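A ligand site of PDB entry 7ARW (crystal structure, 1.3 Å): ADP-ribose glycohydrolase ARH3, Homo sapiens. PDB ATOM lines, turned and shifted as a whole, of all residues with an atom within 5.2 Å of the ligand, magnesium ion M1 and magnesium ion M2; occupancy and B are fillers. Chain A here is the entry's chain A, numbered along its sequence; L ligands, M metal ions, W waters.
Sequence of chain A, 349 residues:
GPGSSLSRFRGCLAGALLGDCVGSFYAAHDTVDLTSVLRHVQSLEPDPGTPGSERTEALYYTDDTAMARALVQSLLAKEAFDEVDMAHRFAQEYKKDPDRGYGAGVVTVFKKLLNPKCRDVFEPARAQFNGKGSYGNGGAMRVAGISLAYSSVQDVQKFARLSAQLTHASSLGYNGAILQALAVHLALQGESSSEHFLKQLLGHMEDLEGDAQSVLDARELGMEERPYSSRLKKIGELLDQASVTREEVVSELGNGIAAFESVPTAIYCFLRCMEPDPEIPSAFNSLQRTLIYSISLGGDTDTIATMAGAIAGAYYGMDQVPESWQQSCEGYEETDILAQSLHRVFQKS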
ATOM      1  N   ASP A  20     -14.915  23.524 -11.057  1.00  0.00           N
ATOM      2  CA  ASP A  20     -13.967  22.425 -11.238  1.00  0.00           C
ATOM      3  C   ASP A  20     -13.955  21.507 -10.017  1.00  0.00           C
ATOM      4  O   ASP A  20     -14.097  20.283 -10.135  1.00  0.00           O
ATOM      5  CB  ASP A  20     -12.582  23.024 -11.501  1.00  0.00           C
ATOM      6  CG  ASP A  20     -11.547  21.998 -11.911  1.00  0.00           C
ATOM      7  OD1 ASP A  20     -11.905  20.860 -12.329  1.00  0.00           O
ATOM      8  OD2 ASP A  20     -10.356  22.331 -11.808  1.00  0.00           O
ATOM      9  N   THR A  62      -8.673  20.135 -10.936  1.00  0.00           N
ATOM     10  CA  THR A  62      -8.191  19.257 -11.999  1.00  0.00           C
ATOM     11  C   THR A  62      -7.411  20.046 -13.042  1.00  0.00           C
ATOM     12  O   THR A  62      -6.984  21.175 -12.779  1.00  0.00           O
ATOM     13  CB  THR A  62      -9.336  18.464 -12.649  1.00  0.00           C
ATOM     14  OG1 THR A  62     -10.116  19.321 -13.511  1.00  0.00           O
ATOM     15  CG2 THR A  62     -10.270  17.874 -11.578  1.00  0.00           C
ATOM     16  N   ASP A  63      -7.219  19.448 -14.219  1.00  0.00           N
ATOM     17  CA  ASP A  63      -6.505  20.127 -15.296  1.00  0.00           C
ATOM     18  C   ASP A  63      -7.149  21.469 -15.661  1.00  0.00           C
ATOM     19  O   ASP A  63      -6.453  22.394 -16.101  1.00  0.00           O
ATOM     20  CB  ASP A  63      -6.394  19.231 -16.526  1.00  0.00           C
ATOM     21  CG  ASP A  63      -7.731  18.846 -17.099  1.00  0.00           C
ATOM     22  OD1 ASP A  63      -8.644  18.499 -16.317  1.00  0.00           O
ATOM     23  OD2 ASP A  63      -7.889  18.890 -18.327  1.00  0.00           O
ATOM     24  N   ASP A  64      -8.476  21.590 -15.499  1.00  0.00           N
ATOM     25  CA  ASP A  64      -9.145  22.858 -15.817  1.00  0.00           C
ATOM     26  C   ASP A  64      -8.482  24.009 -15.075  1.00  0.00           C
ATOM     27  O   ASP A  64      -8.104  25.024 -15.674  1.00  0.00           O
ATOM     28  CB  ASP A  64     -10.628  22.794 -15.429  1.00  0.00           C
ATOM     29  CG  ASP A  64     -11.380  21.718 -16.183  1.00  0.00           C
ATOM     30  OD1 ASP A  64     -11.050  20.527 -16.023  1.00  0.00           O
ATOM     31  OD2 ASP A  64     -12.337  22.062 -16.931  1.00  0.00           O
ATOM     32  N   ARG A 100      -3.442  15.397 -13.265  1.00  0.00           N
ATOM     33  CA  ARG A 100      -4.607  16.201 -12.902  1.00  0.00           C
ATOM     34  C   ARG A 100      -5.853  15.866 -13.711  1.00  0.00           C
ATOM     35  O   ARG A 100      -6.932  16.394 -13.393  1.00  0.00           O
ATOM     36  CB  ARG A 100      -4.292  17.688 -13.061  1.00  0.00           C
ATOM     37  CG  ARG A 100      -3.382  18.223 -11.976  1.00  0.00           C
ATOM     38  CD  ARG A 100      -4.178  18.552 -10.728  1.00  0.00           C
ATOM     39  NE  ARG A 100      -3.337  19.220  -9.736  1.00  0.00           N
ATOM     40  CZ  ARG A 100      -3.742  19.600  -8.533  1.00  0.00           C
ATOM     41  NH1 ARG A 100      -4.972  19.350  -8.109  1.00  0.00           N
ATOM     42  NH2 ARG A 100      -2.884  20.196  -7.705  1.00  0.00           N
ATOM     43  N   GLY A 101      -5.747  15.030 -14.738  1.00  0.00           N
ATOM     44  CA  GLY A 101      -6.920  14.633 -15.510  1.00  0.00           C
ATOM     45  C   GLY A 101      -6.963  15.237 -16.904  1.00  0.00           C
ATOM     46  O   GLY A 101      -8.039  15.504 -17.438  1.00  0.00           O
ATOM     47  N   TYR A 102      -5.798  15.464 -17.499  1.00  0.00           N
ATOM     48  CA  TYR A 102      -5.703  16.040 -18.829  1.00  0.00           C
ATOM     49  C   TYR A 102      -6.344  15.136 -19.882  1.00  0.00           C
ATOM     50  O   TYR A 102      -6.422  13.908 -19.729  1.00  0.00           O
ATOM     51  CB  TYR A 102      -4.236  16.240 -19.187  1.00  0.00           C
ATOM     52  CG  TYR A 102      -3.590  17.375 -18.430  1.00  0.00           C
ATOM     53  CD1 TYR A 102      -3.715  18.694 -18.878  1.00  0.00           C
ATOM     54  CD2 TYR A 102      -2.859  17.138 -17.273  1.00  0.00           C
ATOM     55  CE1 TYR A 102      -3.126  19.730 -18.185  1.00  0.00           C
ATOM     56  CE2 TYR A 102      -2.262  18.184 -16.588  1.00  0.00           C
ATOM     57  CZ  TYR A 102      -2.403  19.467 -17.041  1.00  0.00           C
ATOM     58  OH  TYR A 102      -1.814  20.491 -16.337  1.00  0.00           O
ATOM     59  N   GLY A 103      -6.797  15.757 -20.968  1.00  0.00           N
ATOM     60  CA  GLY A 103      -7.275  14.991 -22.108  1.00  0.00           C
ATOM     61  C   GLY A 103      -6.190  14.112 -22.690  1.00  0.00           C
ATOM     62  O   GLY A 103      -4.999  14.416 -22.619  1.00  0.00           O
ATOM     63  N   ALA A 104      -6.621  12.987 -23.274  1.00  0.00           N
ATOM     64  CA  ALA A 104      -5.651  12.002 -23.759  1.00  0.00           C
ATOM     65  C   ALA A 104      -4.835  12.528 -24.935  1.00  0.00           C
ATOM     66  O   ALA A 104      -3.658  12.162 -25.075  1.00  0.00           O
ATOM     67  CB  ALA A 104      -6.364  10.709 -24.142  1.00  0.00           C
ATOM     68  N   GLY A 105      -5.415  13.369 -25.771  1.00  0.00           N
ATOM     69  CA  GLY A 105      -4.680  13.883 -26.918  1.00  0.00           C
ATOM     70  C   GLY A 105      -3.747  15.030 -26.592  1.00  0.00           C
ATOM     71  O   GLY A 105      -2.622  15.074 -27.096  1.00  0.00           O
ATOM     72  N   VAL A 106      -4.187  15.951 -25.721  1.00  0.00           N
ATOM     73  CA  VAL A 106      -3.417  17.161 -25.472  1.00  0.00           C
ATOM     74  C   VAL A 106      -2.051  16.863 -24.860  1.00  0.00           C
ATOM     75  O   VAL A 106      -1.128  17.675 -25.003  1.00  0.00           O
ATOM     76  CB  VAL A 106      -4.228  18.166 -24.631  1.00  0.00           C
ATOM     77  CG1 VAL A 106      -4.356  17.689 -23.201  1.00  0.00           C
ATOM     78  CG2 VAL A 106      -3.608  19.555 -24.690  1.00  0.00           C
ATOM     79  N   GLN A 128      -2.151  18.004 -34.221  1.00  0.00           N
ATOM     80  CA  GLN A 128      -3.060  17.103 -33.517  1.00  0.00           C
ATOM     81  C   GLN A 128      -4.109  16.544 -34.466  1.00  0.00           C
ATOM     82  O   GLN A 128      -4.620  17.239 -35.351  1.00  0.00           O
ATOM     83  CB  GLN A 128      -3.758  17.859 -32.391  1.00  0.00           C
ATOM     84  CG  GLN A 128      -2.860  18.232 -31.225  1.00  0.00           C
ATOM     85  CD  GLN A 128      -2.447  17.037 -30.400  1.00  0.00           C
ATOM     86  OE1 GLN A 128      -1.527  16.313 -30.779  1.00  0.00           O
ATOM     87  NE2 GLN A 128      -3.141  16.820 -29.296  1.00  0.00           N
ATOM     88  N   PHE A 129      -4.416  15.260 -34.281  1.00  0.00           N
ATOM     89  CA  PHE A 129      -5.507  14.585 -34.991  1.00  0.00           C
ATOM     90  C   PHE A 129      -5.367  14.725 -36.506  1.00  0.00           C
ATOM     91  O   PHE A 129      -6.226  15.283 -37.200  1.00  0.00           O
ATOM     92  CB  PHE A 129      -6.877  15.035 -34.459  1.00  0.00           C
ATOM     93  CG  PHE A 129      -7.034  14.830 -32.980  1.00  0.00           C
ATOM     94  CD1 PHE A 129      -7.231  13.559 -32.472  1.00  0.00           C
ATOM     95  CD2 PHE A 129      -6.947  15.900 -32.099  1.00  0.00           C
ATOM     96  CE1 PHE A 129      -7.371  13.352 -31.106  1.00  0.00           C
ATOM     97  CE2 PHE A 129      -7.059  15.702 -30.732  1.00  0.00           C
ATOM     98  CZ  PHE A 129      -7.281  14.422 -30.234  1.00  0.00           C
ATOM     99  N   LYS A 132      -5.745  18.221 -38.167  1.00  0.00           N
ATOM    100  CA  LYS A 132      -7.003  18.968 -38.107  1.00  0.00           C
ATOM    101  C   LYS A 132      -7.159  19.752 -36.803  1.00  0.00           C
ATOM    102  O   LYS A 132      -7.988  20.673 -36.756  1.00  0.00           O
ATOM    103  CB  LYS A 132      -8.194  18.017 -38.220  1.00  0.00           C
ATOM    104  CG  LYS A 132      -8.161  17.086 -39.428  1.00  0.00           C
ATOM    105  CD  LYS A 132      -8.409  17.812 -40.724  1.00  0.00           C
ATOM    106  CE  LYS A 132      -8.413  16.847 -41.892  1.00  0.00           C
ATOM    107  NZ  LYS A 132      -8.506  17.550 -43.204  1.00  0.00           N
ATOM    108  N   GLY A 133      -6.432  19.389 -35.751  1.00  0.00           N
ATOM    109  CA  GLY A 133      -6.551  20.095 -34.481  1.00  0.00           C
ATOM    110  C   GLY A 133      -7.608  19.474 -33.573  1.00  0.00           C
ATOM    111  O   GLY A 133      -8.578  18.871 -34.023  1.00  0.00           O
ATOM    112  N   SER A 134      -7.396  19.639 -32.278  1.00  0.00           N
ATOM    113  CA  SER A 134      -8.384  19.177 -31.314  1.00  0.00           C
ATOM    114  C   SER A 134      -9.625  20.059 -31.320  1.00  0.00           C
ATOM    115  O   SER A 134      -9.543  21.289 -31.428  1.00  0.00           O
ATOM    116  CB  SER A 134      -7.789  19.200 -29.925  1.00  0.00           C
ATOM    117  OG  SER A 134      -8.772  18.827 -28.976  1.00  0.00           O
ATOM    118  N   TYR A 135     -10.793  19.417 -31.197  1.00  0.00           N
ATOM    119  CA  TYR A 135     -12.043  20.111 -30.955  1.00  0.00           C
ATOM    120  C   TYR A 135     -12.502  20.003 -29.508  1.00  0.00           C
ATOM    121  O   TYR A 135     -13.654  20.311 -29.200  1.00  0.00           O
ATOM    122  CB  TYR A 135     -13.146  19.610 -31.910  1.00  0.00           C
ATOM    123  CG  TYR A 135     -13.407  18.114 -31.924  1.00  0.00           C
ATOM    124  CD1 TYR A 135     -13.758  17.425 -30.770  1.00  0.00           C
ATOM    125  CD2 TYR A 135     -13.325  17.390 -33.110  1.00  0.00           C
ATOM    126  CE1 TYR A 135     -13.999  16.063 -30.781  1.00  0.00           C
ATOM    127  CE2 TYR A 135     -13.582  16.027 -33.140  1.00  0.00           C
ATOM    128  CZ  TYR A 135     -13.912  15.370 -31.968  1.00  0.00           C
ATOM    129  OH  TYR A 135     -14.157  14.021 -31.982  1.00  0.00           O
ATOM    130  N   GLY A 136     -11.619  19.559 -28.612  1.00  0.00           N
ATOM    131  CA  GLY A 136     -11.984  19.426 -27.209  1.00  0.00           C
ATOM    132  C   GLY A 136     -12.219  20.775 -26.555  1.00  0.00           C
ATOM    133  O   GLY A 136     -11.923  21.832 -27.117  1.00  0.00           O
ATOM    134  N   ASN A 137     -12.771  20.721 -25.340  1.00  0.00           N
ATOM    135  CA  ASN A 137     -13.100  21.934 -24.611  1.00  0.00           C
ATOM    136  C   ASN A 137     -11.952  22.487 -23.770  1.00  0.00           C
ATOM    137  O   ASN A 137     -12.147  23.450 -23.032  1.00  0.00           O
ATOM    138  CB  ASN A 137     -14.373  21.752 -23.770  1.00  0.00           C
ATOM    139  CG  ASN A 137     -14.274  20.601 -22.804  1.00  0.00           C
ATOM    140  OD1 ASN A 137     -13.173  20.192 -22.427  1.00  0.00           O
ATOM    141  ND2 ASN A 137     -15.431  20.096 -22.377  1.00  0.00           N
ATOM    142  N   GLY A 138     -10.731  21.949 -23.935  1.00  0.00           N
ATOM    143  CA  GLY A 138      -9.619  22.375 -23.104  1.00  0.00           C
ATOM    144  C   GLY A 138      -9.165  23.800 -23.340  1.00  0.00           C
ATOM    145  O   GLY A 138      -8.634  24.455 -22.432  1.00  0.00           O
ATOM    146  N   GLY A 139      -9.349  24.320 -24.562  1.00  0.00           N
ATOM    147  CA  GLY A 139      -9.042  25.722 -24.797  1.00  0.00           C
ATOM    148  C   GLY A 139      -9.996  26.666 -24.083  1.00  0.00           C
ATOM    149  O   GLY A 139      -9.590  27.744 -23.629  1.00  0.00           O
ATOM    150  N   MET A 141     -11.905  25.750 -21.291  1.00  0.00           N
ATOM    151  CA  MET A 141     -12.004  25.470 -19.859  1.00  0.00           C
ATOM    152  C   MET A 141     -11.117  26.398 -19.036  1.00  0.00           C
ATOM    153  O   MET A 141     -11.391  26.611 -17.853  1.00  0.00           O
ATOM    154  CB  MET A 141     -11.625  24.017 -19.574  1.00  0.00           C
ATOM    155  CG  MET A 141     -10.115  23.760 -19.525  1.00  0.00           C
ATOM    156  SD  MET A 141      -9.752  22.019 -19.342  1.00  0.00           S
ATOM    157  CE  MET A 141      -7.971  22.071 -19.517  1.00  0.00           C
ATOM    158  N   THR A 167      -3.074  24.769 -27.781  1.00  0.00           N
ATOM    159  CA  THR A 167      -3.442  23.359 -27.683  1.00  0.00           C
ATOM    160  C   THR A 167      -4.561  22.966 -28.640  1.00  0.00           C
ATOM    161  O   THR A 167      -4.682  21.771 -28.947  1.00  0.00           O
ATOM    162  CB  THR A 167      -3.859  22.990 -26.247  1.00  0.00           C
ATOM    163  OG1 THR A 167      -4.947  23.828 -25.829  1.00  0.00           O
ATOM    164  CG2 THR A 167      -2.700  23.174 -25.271  1.00  0.00           C
ATOM    165  N   HIS A 168      -5.347  23.915 -29.136  1.00  0.00           N
ATOM    166  CA  HIS A 168      -6.593  23.643 -29.849  1.00  0.00           C
ATOM    167  C   HIS A 168      -6.621  24.445 -31.137  1.00  0.00           C
ATOM    168  O   HIS A 168      -7.038  25.609 -31.148  1.00  0.00           O
ATOM    169  CB  HIS A 168      -7.797  23.955 -28.972  1.00  0.00           C
ATOM    170  CG  HIS A 168      -7.989  22.940 -27.892  1.00  0.00           C
ATOM    171  ND1 HIS A 168      -7.140  22.861 -26.811  1.00  0.00           N
ATOM    172  CD2 HIS A 168      -8.883  21.940 -27.758  1.00  0.00           C
ATOM    173  CE1 HIS A 168      -7.518  21.855 -26.048  1.00  0.00           C
ATOM    174  NE2 HIS A 168      -8.577  21.274 -26.594  1.00  0.00           N
ATOM    175  N   ILE A 257     -17.094  16.239 -24.004  1.00  0.00           N
ATOM    176  CA  ILE A 257     -15.739  16.790 -23.927  1.00  0.00           C
ATOM    177  C   ILE A 257     -15.421  17.706 -25.097  1.00  0.00           C
ATOM    178  O   ILE A 257     -14.412  18.430 -25.055  1.00  0.00           O
ATOM    179  CB  ILE A 257     -14.710  15.642 -23.871  1.00  0.00           C
ATOM    180  CG1 ILE A 257     -14.759  14.801 -25.143  1.00  0.00           C
ATOM    181  CG2 ILE A 257     -14.980  14.777 -22.671  1.00  0.00           C
ATOM    182  CD1 ILE A 257     -13.779  13.641 -25.152  1.00  0.00           C
ATOM    183  N   GLY A 299     -22.200  14.065 -17.721  1.00  0.00           N
ATOM    184  CA  GLY A 299     -21.196  14.199 -18.769  1.00  0.00           C
ATOM    185  C   GLY A 299     -19.912  14.789 -18.221  1.00  0.00           C
ATOM    186  O   GLY A 299     -19.418  14.386 -17.162  1.00  0.00           O
ATOM    187  N   ASP A 300     -19.346  15.771 -18.942  1.00  0.00           N
ATOM    188  CA  ASP A 300     -18.070  16.391 -18.575  1.00  0.00           C
ATOM    189  C   ASP A 300     -18.352  17.470 -17.531  1.00  0.00           C
ATOM    190  O   ASP A 300     -18.224  18.676 -17.760  1.00  0.00           O
ATOM    191  CB  ASP A 300     -17.363  16.932 -19.812  1.00  0.00           C
ATOM    192  CG  ASP A 300     -15.952  17.392 -19.518  1.00  0.00           C
ATOM    193  OD1 ASP A 300     -15.495  17.290 -18.360  1.00  0.00           O
ATOM    194  OD2 ASP A 300     -15.258  17.841 -20.471  1.00  0.00           O
ATOM    195  N   THR A 301     -18.691  17.003 -16.340  1.00  0.00           N
ATOM    196  CA  THR A 301     -19.221  17.897 -15.310  1.00  0.00           C
ATOM    197  C   THR A 301     -18.186  18.912 -14.854  1.00  0.00           C
ATOM    198  O   THR A 301     -18.522  20.080 -14.620  1.00  0.00           O
ATOM    199  CB  THR A 301     -19.769  17.093 -14.129  1.00  0.00           C
ATOM    200  OG1 THR A 301     -18.714  16.319 -13.543  1.00  0.00           O
ATOM    201  CG2 THR A 301     -20.853  16.158 -14.601  1.00  0.00           C
ATOM    202  N   ASP A 302     -16.921  18.517 -14.700  1.00  0.00           N
ATOM    203  CA  ASP A 302     -15.964  19.469 -14.176  1.00  0.00           C
ATOM    204  C   ASP A 302     -15.781  20.647 -15.136  1.00  0.00           C
ATOM    205  O   ASP A 302     -15.664  21.791 -14.696  1.00  0.00           O
ATOM    206  CB  ASP A 302     -14.635  18.810 -13.780  1.00  0.00           C
ATOM    207  CG  ASP A 302     -13.867  18.284 -14.953  1.00  0.00           C
ATOM    208  OD1 ASP A 302     -14.483  17.963 -15.984  1.00  0.00           O
ATOM    209  OD2 ASP A 302     -12.618  18.191 -14.845  1.00  0.00           O
ATOM    210  N   THR A 303     -15.784  20.378 -16.442  1.00  0.00           N
ATOM    211  CA  THR A 303     -15.536  21.469 -17.379  1.00  0.00           C
ATOM    212  C   THR A 303     -16.792  22.284 -17.629  1.00  0.00           C
ATOM    213  O   THR A 303     -16.735  23.523 -17.727  1.00  0.00           O
ATOM    214  CB  THR A 303     -14.923  20.906 -18.653  1.00  0.00           C
ATOM    215  OG1 THR A 303     -13.703  20.217 -18.316  1.00  0.00           O
ATOM    216  CG2 THR A 303     -14.625  22.025 -19.635  1.00  0.00           C
HETATM  217  P1  LIG L   1      -7.885  16.892 -25.962  1.00  0.00           P
HETATM  218  O1  LIG L   1      -7.404  18.000 -26.828  1.00  0.00           O
HETATM  219  O2  LIG L   1      -6.881  15.601 -25.909  1.00  0.00           O
HETATM  220  O3  LIG L   1      -9.320  16.335 -26.493  1.00  0.00           O
HETATM  221  C1  LIG L   1      -9.940  15.398 -25.611  1.00  0.00           C
HETATM  222  C2  LIG L   1     -10.393  14.233 -26.522  1.00  0.00           C
HETATM  223  O4  LIG L   1     -11.349  14.590 -27.512  1.00  0.00           O
HETATM  224  C3  LIG L   1      -9.255  13.568 -27.289  1.00  0.00           C
HETATM  225  O5  LIG L   1      -8.528  12.717 -26.385  1.00  0.00           O
HETATM  226  C4  LIG L   1     -10.100  12.766 -28.341  1.00  0.00           C
HETATM  227  O6  LIG L   1     -10.690  11.603 -27.742  1.00  0.00           O
HETATM  228  C5  LIG L   1     -11.157  13.772 -28.699  1.00  0.00           C
HETATM  229  N1  LIG L   1     -10.834  14.672 -29.768  1.00  0.00           N
HETATM  230  C6  LIG L   1     -10.553  16.022 -29.726  1.00  0.00           C
HETATM  231  N2  LIG L   1     -10.324  16.475 -30.933  1.00  0.00           N
HETATM  232  C7  LIG L   1     -10.467  15.441 -31.809  1.00  0.00           C
HETATM  233  C8  LIG L   1     -10.352  15.266 -33.209  1.00  0.00           C
HETATM  234  N3  LIG L   1     -10.035  16.309 -34.035  1.00  0.00           N
HETATM  235  N4  LIG L   1     -10.554  14.069 -33.707  1.00  0.00           N
HETATM  236  C9  LIG L   1     -10.867  13.013 -32.955  1.00  0.00           C
HETATM  237  N5  LIG L   1     -10.978  13.116 -31.670  1.00  0.00           N
HETATM  238  C10 LIG L   1     -10.797  14.282 -31.059  1.00  0.00           C
HETATM  239  O7  LIG L   1      -7.989  17.426 -24.401  1.00  0.00           O
HETATM  240  P2  LIG L   1      -8.754  18.774 -23.921  1.00  0.00           P
HETATM  241  O8  LIG L   1      -9.649  19.449 -25.000  1.00  0.00           O
HETATM  242  O9  LIG L   1      -7.756  19.711 -23.345  1.00  0.00           O
HETATM  243  O10 LIG L   1      -9.706  18.186 -22.736  1.00  0.00           O
HETATM  244  C11 LIG L   1     -11.056  17.942 -23.103  1.00  0.00           C
HETATM  245  C12 LIG L   1     -11.750  17.412 -21.827  1.00  0.00           C
HETATM  246  O11 LIG L   1     -11.160  16.093 -21.454  1.00  0.00           O
HETATM  247  C13 LIG L   1     -11.580  18.313 -20.591  1.00  0.00           C
HETATM  248  O12 LIG L   1     -12.807  18.275 -19.814  1.00  0.00           O
HETATM  249  C14 LIG L   1     -10.423  17.688 -19.824  1.00  0.00           C
HETATM  250  O13 LIG L   1     -10.559  17.978 -18.462  1.00  0.00           O
HETATM  251  C15 LIG L   1     -10.556  16.166 -20.130  1.00  0.00           C
HETATM  252  N6  LIG L   1     -11.405  15.447 -19.123  1.00  0.00           N
HETATM  253  C16 LIG L   1     -12.702  15.046 -19.413  1.00  0.00           C
HETATM  254  C17 LIG L   1     -13.477  14.384 -18.496  1.00  0.00           C
HETATM  255  C18 LIG L   1     -14.791  13.969 -18.793  1.00  0.00           C
HETATM  256  O14 LIG L   1     -15.239  13.990 -19.953  1.00  0.00           O
HETATM  257  N7  LIG L   1     -15.586  13.514 -17.787  1.00  0.00           N
HETATM  258  C19 LIG L   1     -12.939  14.076 -17.093  1.00  0.00           C
HETATM  259  C20 LIG L   1     -11.528  14.571 -16.888  1.00  0.00           C
HETATM  260  C21 LIG L   1     -10.847  15.204 -17.846  1.00  0.00           C
HETATM  261 MG    MG M   1     -10.855  18.478 -15.722  1.00  0.00          MG
HETATM  262 MG    MG M   2     -13.509  17.868 -17.703  1.00  0.00          MG
HETATM  263  O   HOH W   1      -6.072  21.694 -22.956  1.00  0.00           O
HETATM  264  O   HOH W   2      -6.725  18.630 -20.851  1.00  0.00           O
HETATM  265  O   HOH W   3     -11.938  10.694 -30.191  1.00  0.00           O
HETATM  266  O   HOH W   4     -10.698  15.751 -36.755  1.00  0.00           O
HETATM  267  O   HOH W   5     -10.031  10.634 -25.016  1.00  0.00           O
HETATM  268  O   HOH W   6     -10.714  18.764 -35.972  1.00  0.00           O
HETATM  269  O   HOH W   7     -10.266  12.744 -36.306  1.00  0.00           O
HETATM  270  O   HOH W   8     -10.134  16.664 -15.241  1.00  0.00           O
HETATM  271  O   HOH W   9      -9.295  12.139 -23.151  1.00  0.00           O
HETATM  272  O   HOH W  10     -15.782  15.710 -15.656  1.00  0.00           O
HETATM  273  O   HOH W  11      -6.818  11.286 -28.204  1.00  0.00           O
HETATM  274  O   HOH W  12      -4.950  18.856 -28.117  1.00  0.00           O
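Water W11 bridges O5 of the ligand and N of Gly 105. Water W12 lies within hydrogen-bond range of an oxygen (O1) of the ligand (2.9 Å), the side-chain amide nitrogen of Gln 128 (3.0 Å) and the backbone carbonyl oxygen of Thr 167 (3.0 Å). Water W2 lies within hydrogen-bond range of OD2 of Asp 63 (2.8 Å), N of Gly 103 (2.9 Å) and O9 of the ligand (2.9 Å). Water W6 lies within hydrogen-bond range of O of Gly 133 (2.9 Å), N3 of the ligand (3.2 Å) and O of Lys 132 (3.4 Å). Water W9 bridges N of Ala 104 (2.8 Å) and O5 of the ligand (3.4 Å).
Magnesium ion M2 is bound by OD1 of Asp 302. Magnesium ion M2 is bound by OD1 of Asp 300 (2.2 Å). Magnesium ion M2 is bound by O12 of the ligand (2.3 Å). Magnesium ion M2 is bound by the side-chain hydroxyl (OG1) of Thr 303 (2.4 Å). Magnesium ion M2 has four donor atoms within binding distance.
The backbone NH of Tyr 135 sits at hydrogen-bond distance from a nitrogen (N2) of the ligand (3.0 Å). The backbone NH (N) of Gly 105 sits at hydrogen-bond distance from an oxygen (O2) of the ligand, at 2.7 Å. O12 of the ligand lies close to OD1 of Asn 137 (3.3 Å). An oxygen (O8) of the ligand is in hydrogen-bond range of the backbone NH of Asn 137, at 3.4 Å. The side-chain carboxylate (OD2) of Asp 63 sits at hydrogen-bond distance from an oxygen (O13) of the ligand (2.8 Å). N5 of the ligand sits at hydrogen-bond distance from OH of Tyr 135 (3.3 Å). An oxygen (O8) of the ligand lies within hydrogen-bond range of the backbone NH of Gly 138 (2.9 Å). O2 of the ligand lies within hydrogen-bond range of N of Val 106 (2.7 Å). An oxygen (O1) of the ligand lies within hydrogen-bond range of the side-chain hydroxyl (OG) of Ser 134. The backbone carbonyl oxygen (O) of Gly 133 lies within hydrogen-bond range of a nitrogen (N3) of the ligand, 2.9 Å away. A ring nitrogen (NE2) of His 168 lies within hydrogen-bond range of an oxygen (O8) of the ligand (2.6 Å).
Magnesium ion M1 is bound by the side-chain carboxylate of Asp 302 (2.0 Å), water W8 (2.0 Å), the side-chain carboxylate of Asp 64 (2.1 Å), the side-chain carboxylate of Asp 63 (2.3 Å) and the side-chain hydroxyl of Thr 62 (2.5 Å). Slightly farther from magnesium ion M1 lies an oxygen (O13) of the ligand (2.8 Å).
N of Asn 137 is in hydrogen-bond range of O of Ile 257, 2.8 Å away. ND1 of His 168 lies close to N of Gly 139, at 3.5 Å. The side-chain hydroxyl (OG) of Ser 134 sits at hydrogen-bond distance from the backbone NH (N) of Gly 136 (3.0 Å). The backbone carbonyl oxygen (O) of Gly 105 sits at hydrogen-bond distance from the side-chain amide nitrogen (NE2) of Gln 128 (2.9 Å). The side-chain hydroxyl of Thr 167 lies within hydrogen-bond range of a ring nitrogen (ND1) of His 168. O of Arg 100 lies within hydrogen-bond range of N of Asp 63. A ring nitrogen (NE2) of His 168 lies within hydrogen-bond range of the backbone NH of Gly 138 (3.5 Å). O of Gly 136 sits close to NE2 of His 168 (3.4 Å).
Four residues have an atom within 4 Å of magnesium ion M2: Asp 64, Asp 300, Asp 302 and Thr 303.
O of Gly 101 touches C21 of the ligand, at 2.9 Å. CA of Gly 103 touches O7 of the ligand, at 3.4 Å. Ala 104 touches the ligand. Phe 129 touches the ligand. CA of Gly 136 touches O8 of the ligand, 3.2 Å away. CG2 of Ile 257 touches O14 of the ligand, 2.8 Å away. Gly 299 touches the ligand. Hydrophobic or aromatic side chains within 4 Å of the ligand: Ala 104, Val 106, Phe 129, Tyr 135, His 168 and Ile 257. Of the 30 residues printed, 19 come within 4 Å of the ligand.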
